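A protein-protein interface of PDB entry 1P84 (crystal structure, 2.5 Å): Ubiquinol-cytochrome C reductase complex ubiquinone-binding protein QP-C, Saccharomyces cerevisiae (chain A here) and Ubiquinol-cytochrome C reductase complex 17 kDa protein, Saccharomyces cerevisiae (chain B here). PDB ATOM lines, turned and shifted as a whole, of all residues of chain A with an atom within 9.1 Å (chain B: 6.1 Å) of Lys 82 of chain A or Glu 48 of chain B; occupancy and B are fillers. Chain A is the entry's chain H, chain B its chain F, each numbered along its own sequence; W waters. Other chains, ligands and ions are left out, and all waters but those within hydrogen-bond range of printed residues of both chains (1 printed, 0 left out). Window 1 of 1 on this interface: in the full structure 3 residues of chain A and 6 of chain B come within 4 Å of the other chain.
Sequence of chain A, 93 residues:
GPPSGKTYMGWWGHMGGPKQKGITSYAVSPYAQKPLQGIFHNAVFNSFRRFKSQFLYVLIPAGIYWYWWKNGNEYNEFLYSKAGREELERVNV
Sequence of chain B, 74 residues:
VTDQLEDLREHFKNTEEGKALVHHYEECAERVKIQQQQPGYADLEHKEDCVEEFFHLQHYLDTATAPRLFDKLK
Of chain B, only Cys 28, Glu 48, Asp 49, Glu 52 and Glu 53 come within 4 Å of Lys 82 of chain A. Of chain A, only Lys 82 comes within 4 Å of Glu 48 of chain B. Of chain A, only Lys 82 comes within 4 Å of Asp 49 of chain B. Printed residues of chain A within 4 Å of Cys 28 of chain B: Lys 82 (3.7 Å). Of the printed residues of chain A, Glu 53 of chain B touches Lys 82. Of the printed residues of chain A, Glu 52 of chain B touches Ser 81 (3.6 Å) and Lys 82 (2.9 Å). Printed residues of chain B within 4 Å of Ser 81 of chain A: Glu 52 (3.6 Å). Glu 87 of chain A touches none of the printed residues of chain B. The nearest printed residue of chain A that does not touch Cys 28 of chain B is Ala 83 of chain A (11.2 Å).
The side-chain amino group of Lys 82 of chain A sits at hydrogen-bond distance from the side-chain sulfur of Cys 28 of chain B (3.7 Å). A ring nitrogen (NE2) of His 46 of chain B sits at hydrogen-bond distance from the guanidinium group of Arg 85 of chain A, at 3.1 Å. The side-chain carboxylate of Glu 48 of chain B is in salt-bridge range of the side-chain amino group of Lys 82 of chain A, 3.1 Å away. The backbone carbonyl oxygen of Asp 49 of chain B lies within hydrogen-bond range of the side-chain amino group of Lys 82 of chain A (2.7 Å). The side-chain carboxylate (OE2) of Glu 52 of chain B lies within hydrogen-bond range of the backbone NH (N) of Lys 82 of chain A. The side-chain amino group (NZ) of Lys 82 of chain A lies within salt-bridge range of the side-chain carboxylate (OE2) of Glu 53 of chain B (2.7 Å).
Among the printed residues, merely in contact across the chains: Ser 81 of chain A with Glu 52 of chain B.
Water W1 lies within hydrogen-bond range of N of Ala 83 of chain A (2.7 Å), OE1 of Glu 52 of chain B (2.7 Å) and N of Lys 82 of chain A (3.1 Å).
Of the 13 printed residues of chain B, 6 touch a printed residue of chain A. Printed residues of chain A that touch a printed residue of chain B: Ser 81, Lys 82 and Arg 85. Among the printed residues, 7 pairs touch across the chains. Among the printed residues, Asp or Glu carboxylates within 4 Å of a Lys or Arg side-chain nitrogen of the other chain: Lys 82 of chain A with Glu 48 of chain B and Lys 82 of chain A with Glu 53 of chain B.
The side-chain sulfur (SG) of Cys 28 of chain B lies within hydrogen-bond range of the guanidinium group (NH1) of Arg 31 of chain B (3.8 Å). SG of Cys 28 of chain B forms a disulfide with SG of Cys 50 of chain B (2.0 Å). The guanidinium group (NH1) of Arg 31 of chain B lies within salt-bridge range of the side-chain carboxylate (OE2) of Glu 48 of chain B (3.0 Å). The side-chain carboxylate (OD2) of Asp 49 of chain B sits close to the backbone NH (N) of Val 51 of chain B. The side-chain hydroxyl (OG) of Ser 81 of chain A is in hydrogen-bond range of the backbone carbonyl oxygen (O) of Phe 78 of chain A (2.7 Å).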
ATOM      1  N   ASN A  76      14.571  28.813   7.033  1.00  0.00           N
ATOM      2  CA  ASN A  76      14.478  28.525   8.464  1.00  0.00           C
ATOM      3  C   ASN A  76      14.737  27.045   8.733  1.00  0.00           C
ATOM      4  O   ASN A  76      15.471  26.685   9.656  1.00  0.00           O
ATOM      5  CB  ASN A  76      13.088  28.907   8.997  1.00  0.00           C
ATOM      6  CG  ASN A  76      12.928  28.619  10.485  1.00  0.00           C
ATOM      7  OD1 ASN A  76      12.257  27.666  10.877  1.00  0.00           O
ATOM      8  ND2 ASN A  76      13.559  29.435  11.317  1.00  0.00           N
ATOM      9  N   GLU A  77      14.115  26.203   7.915  1.00  0.00           N
ATOM     10  CA  GLU A  77      14.228  24.758   8.016  1.00  0.00           C
ATOM     11  C   GLU A  77      15.690  24.341   7.895  1.00  0.00           C
ATOM     12  O   GLU A  77      16.191  23.545   8.696  1.00  0.00           O
ATOM     13  CB  GLU A  77      13.393  24.126   6.910  1.00  0.00           C
ATOM     14  CG  GLU A  77      13.023  22.678   7.138  1.00  0.00           C
ATOM     15  CD  GLU A  77      11.842  22.257   6.281  1.00  0.00           C
ATOM     16  OE1 GLU A  77      10.702  22.660   6.619  1.00  0.00           O
ATOM     17  OE2 GLU A  77      12.054  21.542   5.269  1.00  0.00           O
ATOM     18  N   PHE A  78      16.374  24.908   6.904  1.00  0.00           N
ATOM     19  CA  PHE A  78      17.780  24.621   6.681  1.00  0.00           C
ATOM     20  C   PHE A  78      18.621  25.037   7.892  1.00  0.00           C
ATOM     21  O   PHE A  78      19.401  24.246   8.411  1.00  0.00           O
ATOM     22  CB  PHE A  78      18.262  25.338   5.419  1.00  0.00           C
ATOM     23  CG  PHE A  78      19.759  25.425   5.301  1.00  0.00           C
ATOM     24  CD1 PHE A  78      20.496  24.359   4.800  1.00  0.00           C
ATOM     25  CD2 PHE A  78      20.438  26.581   5.708  1.00  0.00           C
ATOM     26  CE1 PHE A  78      21.892  24.438   4.707  1.00  0.00           C
ATOM     27  CE2 PHE A  78      21.827  26.672   5.620  1.00  0.00           C
ATOM     28  CZ  PHE A  78      22.560  25.598   5.119  1.00  0.00           C
ATOM     29  N   LEU A  79      18.442  26.268   8.351  1.00  0.00           N
ATOM     30  CA  LEU A  79      19.192  26.778   9.492  1.00  0.00           C
ATOM     31  C   LEU A  79      19.139  25.880  10.724  1.00  0.00           C
ATOM     32  O   LEU A  79      20.122  25.770  11.457  1.00  0.00           O
ATOM     33  CB  LEU A  79      18.696  28.175   9.879  1.00  0.00           C
ATOM     34  CG  LEU A  79      18.966  29.368   8.964  1.00  0.00           C
ATOM     35  CD1 LEU A  79      18.352  30.604   9.582  1.00  0.00           C
ATOM     36  CD2 LEU A  79      20.453  29.574   8.790  1.00  0.00           C
ATOM     37  N   TYR A  80      18.000  25.234  10.953  1.00  0.00           N
ATOM     38  CA  TYR A  80      17.851  24.385  12.130  1.00  0.00           C
ATOM     39  C   TYR A  80      18.083  22.895  11.913  1.00  0.00           C
ATOM     40  O   TYR A  80      17.830  22.080  12.804  1.00  0.00           O
ATOM     41  CB  TYR A  80      16.518  24.668  12.840  1.00  0.00           C
ATOM     42  CG  TYR A  80      16.523  26.000  13.559  1.00  0.00           C
ATOM     43  CD1 TYR A  80      16.325  27.196  12.859  1.00  0.00           C
ATOM     44  CD2 TYR A  80      16.797  26.075  14.926  1.00  0.00           C
ATOM     45  CE1 TYR A  80      16.411  28.429  13.502  1.00  0.00           C
ATOM     46  CE2 TYR A  80      16.882  27.297  15.573  1.00  0.00           C
ATOM     47  CZ  TYR A  80      16.691  28.466  14.856  1.00  0.00           C
ATOM     48  OH  TYR A  80      16.791  29.672  15.498  1.00  0.00           O
ATOM     49  N   SER A  81      18.558  22.539  10.722  1.00  0.00           N
ATOM     50  CA  SER A  81      18.881  21.151  10.424  1.00  0.00           C
ATOM     51  C   SER A  81      20.366  20.993  10.757  1.00  0.00           C
ATOM     52  O   SER A  81      20.996  21.929  11.264  1.00  0.00           O
ATOM     53  CB  SER A  81      18.616  20.821   8.951  1.00  0.00           C
ATOM     54  OG  SER A  81      19.467  21.546   8.087  1.00  0.00           O
ATOM     55  N   LYS A  82      20.922  19.814  10.496  1.00  0.00           N
ATOM     56  CA  LYS A  82      22.333  19.568  10.785  1.00  0.00           C
ATOM     57  C   LYS A  82      23.216  20.382   9.848  1.00  0.00           C
ATOM     58  O   LYS A  82      24.088  21.126  10.295  1.00  0.00           O
ATOM     59  CB  LYS A  82      22.651  18.081  10.631  1.00  0.00           C
ATOM     60  CG  LYS A  82      23.178  17.435  11.890  1.00  0.00           C
ATOM     61  CD  LYS A  82      23.347  15.943  11.700  1.00  0.00           C
ATOM     62  CE  LYS A  82      23.701  15.279  13.009  1.00  0.00           C
ATOM     63  NZ  LYS A  82      23.590  13.804  12.899  1.00  0.00           N
ATOM     64  N   ALA A  83      22.948  20.256   8.552  1.00  0.00           N
ATOM     65  CA  ALA A  83      23.694  20.939   7.508  1.00  0.00           C
ATOM     66  C   ALA A  83      23.892  22.434   7.733  1.00  0.00           C
ATOM     67  O   ALA A  83      24.941  22.988   7.389  1.00  0.00           O
ATOM     68  CB  ALA A  83      23.022  20.702   6.161  1.00  0.00           C
ATOM     69  N   GLY A  84      22.901  23.083   8.334  1.00  0.00           N
ATOM     70  CA  GLY A  84      22.990  24.514   8.550  1.00  0.00           C
ATOM     71  C   GLY A  84      23.377  25.028   9.919  1.00  0.00           C
ATOM     72  O   GLY A  84      23.366  26.240  10.130  1.00  0.00           O
ATOM     73  N   ARG A  85      23.743  24.146  10.842  1.00  0.00           N
ATOM     74  CA  ARG A  85      24.117  24.588  12.185  1.00  0.00           C
ATOM     75  C   ARG A  85      25.334  25.516  12.185  1.00  0.00           C
ATOM     76  O   ARG A  85      25.574  26.244  13.150  1.00  0.00           O
ATOM     77  CB  ARG A  85      24.350  23.394  13.121  1.00  0.00           C
ATOM     78  CG  ARG A  85      25.521  22.501  12.750  1.00  0.00           C
ATOM     79  CD  ARG A  85      25.986  21.697  13.962  1.00  0.00           C
ATOM     80  NE  ARG A  85      26.235  22.570  15.113  1.00  0.00           N
ATOM     81  CZ  ARG A  85      27.186  23.503  15.168  1.00  0.00           C
ATOM     82  NH1 ARG A  85      27.317  24.250  16.259  1.00  0.00           N
ATOM     83  NH2 ARG A  85      28.024  23.680  14.149  1.00  0.00           N
ATOM     84  N   GLU A  86      26.089  25.490  11.090  1.00  0.00           N
ATOM     85  CA  GLU A  86      27.274  26.329  10.945  1.00  0.00           C
ATOM     86  C   GLU A  86      26.836  27.746  10.566  1.00  0.00           C
ATOM     87  O   GLU A  86      27.241  28.718  11.206  1.00  0.00           O
ATOM     88  CB  GLU A  86      28.212  25.737   9.887  1.00  0.00           C
ATOM     89  CG  GLU A  86      29.664  26.191  10.016  1.00  0.00           C
ATOM     90  CD  GLU A  86      30.606  25.411   9.113  1.00  0.00           C
ATOM     91  OE1 GLU A  86      30.829  25.844   7.956  1.00  0.00           O
ATOM     92  OE2 GLU A  86      31.124  24.364   9.565  1.00  0.00           O
ATOM     93  N   GLU A  87      25.989  27.854   9.541  1.00  0.00           N
ATOM     94  CA  GLU A  87      25.477  29.151   9.109  1.00  0.00           C
ATOM     95  C   GLU A  87      24.571  29.750  10.186  1.00  0.00           C
ATOM     96  O   GLU A  87      24.471  30.968  10.310  1.00  0.00           O
ATOM     97  CB  GLU A  87      24.718  29.034   7.781  1.00  0.00           C
ATOM     98  CG  GLU A  87      23.916  30.286   7.431  1.00  0.00           C
ATOM     99  CD  GLU A  87      24.015  30.678   5.972  1.00  0.00           C
ATOM    100  OE1 GLU A  87      23.166  30.235   5.166  1.00  0.00           O
ATOM    101  OE2 GLU A  87      24.938  31.453   5.633  1.00  0.00           O
ATOM    102  N   LEU A  88      23.937  28.885  10.975  1.00  0.00           N
ATOM    103  CA  LEU A  88      23.050  29.321  12.052  1.00  0.00           C
ATOM    104  C   LEU A  88      23.836  30.111  13.094  1.00  0.00           C
ATOM    105  O   LEU A  88      23.356  31.121  13.586  1.00  0.00           O
ATOM    106  CB  LEU A  88      22.342  28.116  12.695  1.00  0.00           C
ATOM    107  CG  LEU A  88      21.272  28.277  13.789  1.00  0.00           C
ATOM    108  CD1 LEU A  88      21.890  28.468  15.163  1.00  0.00           C
ATOM    109  CD2 LEU A  88      20.339  29.416  13.446  1.00  0.00           C
ATOM    110  N   CYS B  28      25.728   7.022  11.000  1.00  0.00           N
ATOM    111  CA  CYS B  28      25.787   8.097  11.984  1.00  0.00           C
ATOM    112  C   CYS B  28      26.153   7.539  13.352  1.00  0.00           C
ATOM    113  O   CYS B  28      27.038   8.067  14.016  1.00  0.00           O
ATOM    114  CB  CYS B  28      24.457   8.848  12.077  1.00  0.00           C
ATOM    115  SG  CYS B  28      24.484  10.259  13.246  1.00  0.00           S
ATOM    116  N   ARG B  31      29.850   6.661  13.453  1.00  0.00           N
ATOM    117  CA  ARG B  31      30.634   7.885  13.553  1.00  0.00           C
ATOM    118  C   ARG B  31      30.589   8.490  14.963  1.00  0.00           C
ATOM    119  O   ARG B  31      31.558   9.097  15.415  1.00  0.00           O
ATOM    120  CB  ARG B  31      30.116   8.894  12.520  1.00  0.00           C
ATOM    121  CG  ARG B  31      30.899  10.194  12.428  1.00  0.00           C
ATOM    122  CD  ARG B  31      30.469  11.035  11.226  1.00  0.00           C
ATOM    123  NE  ARG B  31      29.090  11.509  11.329  1.00  0.00           N
ATOM    124  CZ  ARG B  31      28.100  11.133  10.520  1.00  0.00           C
ATOM    125  NH1 ARG B  31      26.878  11.623  10.692  1.00  0.00           N
ATOM    126  NH2 ARG B  31      28.326  10.259   9.545  1.00  0.00           N
ATOM    127  N   VAL B  32      29.481   8.276  15.670  1.00  0.00           N
ATOM    128  CA  VAL B  32      29.299   8.810  17.018  1.00  0.00           C
ATOM    129  C   VAL B  32      30.069   8.083  18.118  1.00  0.00           C
ATOM    130  O   VAL B  32      30.742   8.728  18.920  1.00  0.00           O
ATOM    131  CB  VAL B  32      27.797   8.875  17.408  1.00  0.00           C
ATOM    132  CG1 VAL B  32      27.637   9.337  18.854  1.00  0.00           C
ATOM    133  CG2 VAL B  32      27.059   9.827  16.485  1.00  0.00           C
ATOM    134  N   GLN B  35      33.610   8.955  18.299  1.00  0.00           N
ATOM    135  CA  GLN B  35      33.850  10.279  18.870  1.00  0.00           C
ATOM    136  C   GLN B  35      33.792  10.273  20.398  1.00  0.00           C
ATOM    137  O   GLN B  35      34.398  11.125  21.050  1.00  0.00           O
ATOM    138  CB  GLN B  35      32.827  11.288  18.342  1.00  0.00           C
ATOM    139  CG  GLN B  35      32.898  11.562  16.847  1.00  0.00           C
ATOM    140  CD  GLN B  35      31.878  12.597  16.394  1.00  0.00           C
ATOM    141  OE1 GLN B  35      31.208  13.230  17.216  1.00  0.00           O
ATOM    142  NE2 GLN B  35      31.756  12.774  15.080  1.00  0.00           N
ATOM    143  N   TYR B  41      35.669  13.991  25.115  1.00  0.00           N
ATOM    144  CA  TYR B  41      34.287  13.990  24.645  1.00  0.00           C
ATOM    145  C   TYR B  41      33.414  14.766  25.625  1.00  0.00           C
ATOM    146  O   TYR B  41      32.507  15.496  25.216  1.00  0.00           O
ATOM    147  CB  TYR B  41      33.754  12.560  24.488  1.00  0.00           C
ATOM    148  CG  TYR B  41      32.336  12.496  23.950  1.00  0.00           C
ATOM    149  CD1 TYR B  41      31.277  12.083  24.761  1.00  0.00           C
ATOM    150  CD2 TYR B  41      32.050  12.867  22.636  1.00  0.00           C
ATOM    151  CE1 TYR B  41      29.971  12.044  24.276  1.00  0.00           C
ATOM    152  CE2 TYR B  41      30.746  12.832  22.141  1.00  0.00           C
ATOM    153  CZ  TYR B  41      29.715  12.421  22.967  1.00  0.00           C
ATOM    154  OH  TYR B  41      28.430  12.389  22.479  1.00  0.00           O
ATOM    155  N   HIS B  46      29.942  20.362  21.142  1.00  0.00           N
ATOM    156  CA  HIS B  46      29.683  20.151  19.725  1.00  0.00           C
ATOM    157  C   HIS B  46      29.367  18.672  19.509  1.00  0.00           C
ATOM    158  O   HIS B  46      29.509  18.153  18.401  1.00  0.00           O
ATOM    159  CB  HIS B  46      30.926  20.543  18.917  1.00  0.00           C
ATOM    160  CG  HIS B  46      30.624  21.301  17.661  1.00  0.00           C
ATOM    161  ND1 HIS B  46      30.481  20.685  16.434  1.00  0.00           N
ATOM    162  CD2 HIS B  46      30.470  22.628  17.435  1.00  0.00           C
ATOM    163  CE1 HIS B  46      30.255  21.601  15.508  1.00  0.00           C
ATOM    164  NE2 HIS B  46      30.243  22.788  16.089  1.00  0.00           N
ATOM    165  N   LYS B  47      28.935  18.006  20.578  1.00  0.00           N
ATOM    166  CA  LYS B  47      28.597  16.586  20.542  1.00  0.00           C
ATOM    167  C   LYS B  47      27.468  16.309  19.557  1.00  0.00           C
ATOM    168  O   LYS B  47      26.375  16.860  19.675  1.00  0.00           O
ATOM    169  CB  LYS B  47      28.198  16.093  21.936  1.00  0.00           C
ATOM    170  CG  LYS B  47      29.189  16.450  23.039  1.00  0.00           C
ATOM    171  CD  LYS B  47      28.825  15.759  24.351  1.00  0.00           C
ATOM    172  CE  LYS B  47      28.886  16.713  25.542  1.00  0.00           C
ATOM    173  NZ  LYS B  47      30.232  17.312  25.741  1.00  0.00           N
ATOM    174  N   GLU B  48      27.750  15.454  18.581  1.00  0.00           N
ATOM    175  CA  GLU B  48      26.779  15.101  17.558  1.00  0.00           C
ATOM    176  C   GLU B  48      25.885  13.946  17.994  1.00  0.00           C
ATOM    177  O   GLU B  48      26.314  13.062  18.739  1.00  0.00           O
ATOM    178  CB  GLU B  48      27.508  14.732  16.261  1.00  0.00           C
ATOM    179  CG  GLU B  48      26.596  14.407  15.080  1.00  0.00           C
ATOM    180  CD  GLU B  48      27.355  14.024  13.816  1.00  0.00           C
ATOM    181  OE1 GLU B  48      28.604  14.033  13.827  1.00  0.00           O
ATOM    182  OE2 GLU B  48      26.700  13.707  12.802  1.00  0.00           O
ATOM    183  N   ASP B  49      24.622  14.004  17.574  1.00  0.00           N
ATOM    184  CA  ASP B  49      23.662  12.949  17.860  1.00  0.00           C
ATOM    185  C   ASP B  49      23.050  12.528  16.537  1.00  0.00           C
ATOM    186  O   ASP B  49      23.257  13.178  15.519  1.00  0.00           O
ATOM    187  CB  ASP B  49      22.589  13.384  18.872  1.00  0.00           C
ATOM    188  CG  ASP B  49      21.840  14.629  18.450  1.00  0.00           C
ATOM    189  OD1 ASP B  49      21.884  15.617  19.215  1.00  0.00           O
ATOM    190  OD2 ASP B  49      21.187  14.619  17.379  1.00  0.00           O
ATOM    191  N   CYS B  50      22.307  11.434  16.546  1.00  0.00           N
ATOM    192  CA  CYS B  50      21.709  10.938  15.321  1.00  0.00           C
ATOM    193  C   CYS B  50      20.192  11.034  15.299  1.00  0.00           C
ATOM    194  O   CYS B  50      19.523  10.307  14.560  1.00  0.00           O
ATOM    195  CB  CYS B  50      22.189   9.510  15.073  1.00  0.00           C
ATOM    196  SG  CYS B  50      24.010   9.416  15.034  1.00  0.00           S
ATOM    197  N   VAL B  51      19.663  11.978  16.076  1.00  0.00           N
ATOM    198  CA  VAL B  51      18.225  12.209  16.163  1.00  0.00           C
ATOM    199  C   VAL B  51      17.660  12.537  14.790  1.00  0.00           C
ATOM    200  O   VAL B  51      16.673  11.948  14.366  1.00  0.00           O
ATOM    201  CB  VAL B  51      17.900  13.364  17.127  1.00  0.00           C
ATOM    202  CG1 VAL B  51      16.402  13.550  17.239  1.00  0.00           C
ATOM    203  CG2 VAL B  51      18.486  13.090  18.492  1.00  0.00           C
ATOM    204  N   GLU B  52      18.322  13.447  14.083  1.00  0.00           N
ATOM    205  CA  GLU B  52      17.878  13.858  12.759  1.00  0.00           C
ATOM    206  C   GLU B  52      17.742  12.656  11.838  1.00  0.00           C
ATOM    207  O   GLU B  52      16.707  12.469  11.202  1.00  0.00           O
ATOM    208  CB  GLU B  52      18.839  14.882  12.168  1.00  0.00           C
ATOM    209  CG  GLU B  52      18.389  15.457  10.843  1.00  0.00           C
ATOM    210  CD  GLU B  52      19.067  16.781  10.522  1.00  0.00           C
ATOM    211  OE1 GLU B  52      19.437  16.997   9.348  1.00  0.00           O
ATOM    212  OE2 GLU B  52      19.220  17.616  11.442  1.00  0.00           O
ATOM    213  N   GLU B  53      18.777  11.819  11.811  1.00  0.00           N
ATOM    214  CA  GLU B  53      18.786  10.609  10.984  1.00  0.00           C
ATOM    215  C   GLU B  53      17.742   9.604  11.478  1.00  0.00           C
ATOM    216  O   GLU B  53      17.116   8.914  10.676  1.00  0.00           O
ATOM    217  CB  GLU B  53      20.181   9.967  10.976  1.00  0.00           C
ATOM    218  CG  GLU B  53      21.271  10.797  10.286  1.00  0.00           C
ATOM    219  CD  GLU B  53      21.824  11.929  11.150  1.00  0.00           C
ATOM    220  OE1 GLU B  53      21.481  12.021  12.352  1.00  0.00           O
ATOM    221  OE2 GLU B  53      22.628  12.726  10.622  1.00  0.00           O
HETATM  222  O   HOH W   1      21.422  18.182   7.889  1.00  0.00           O
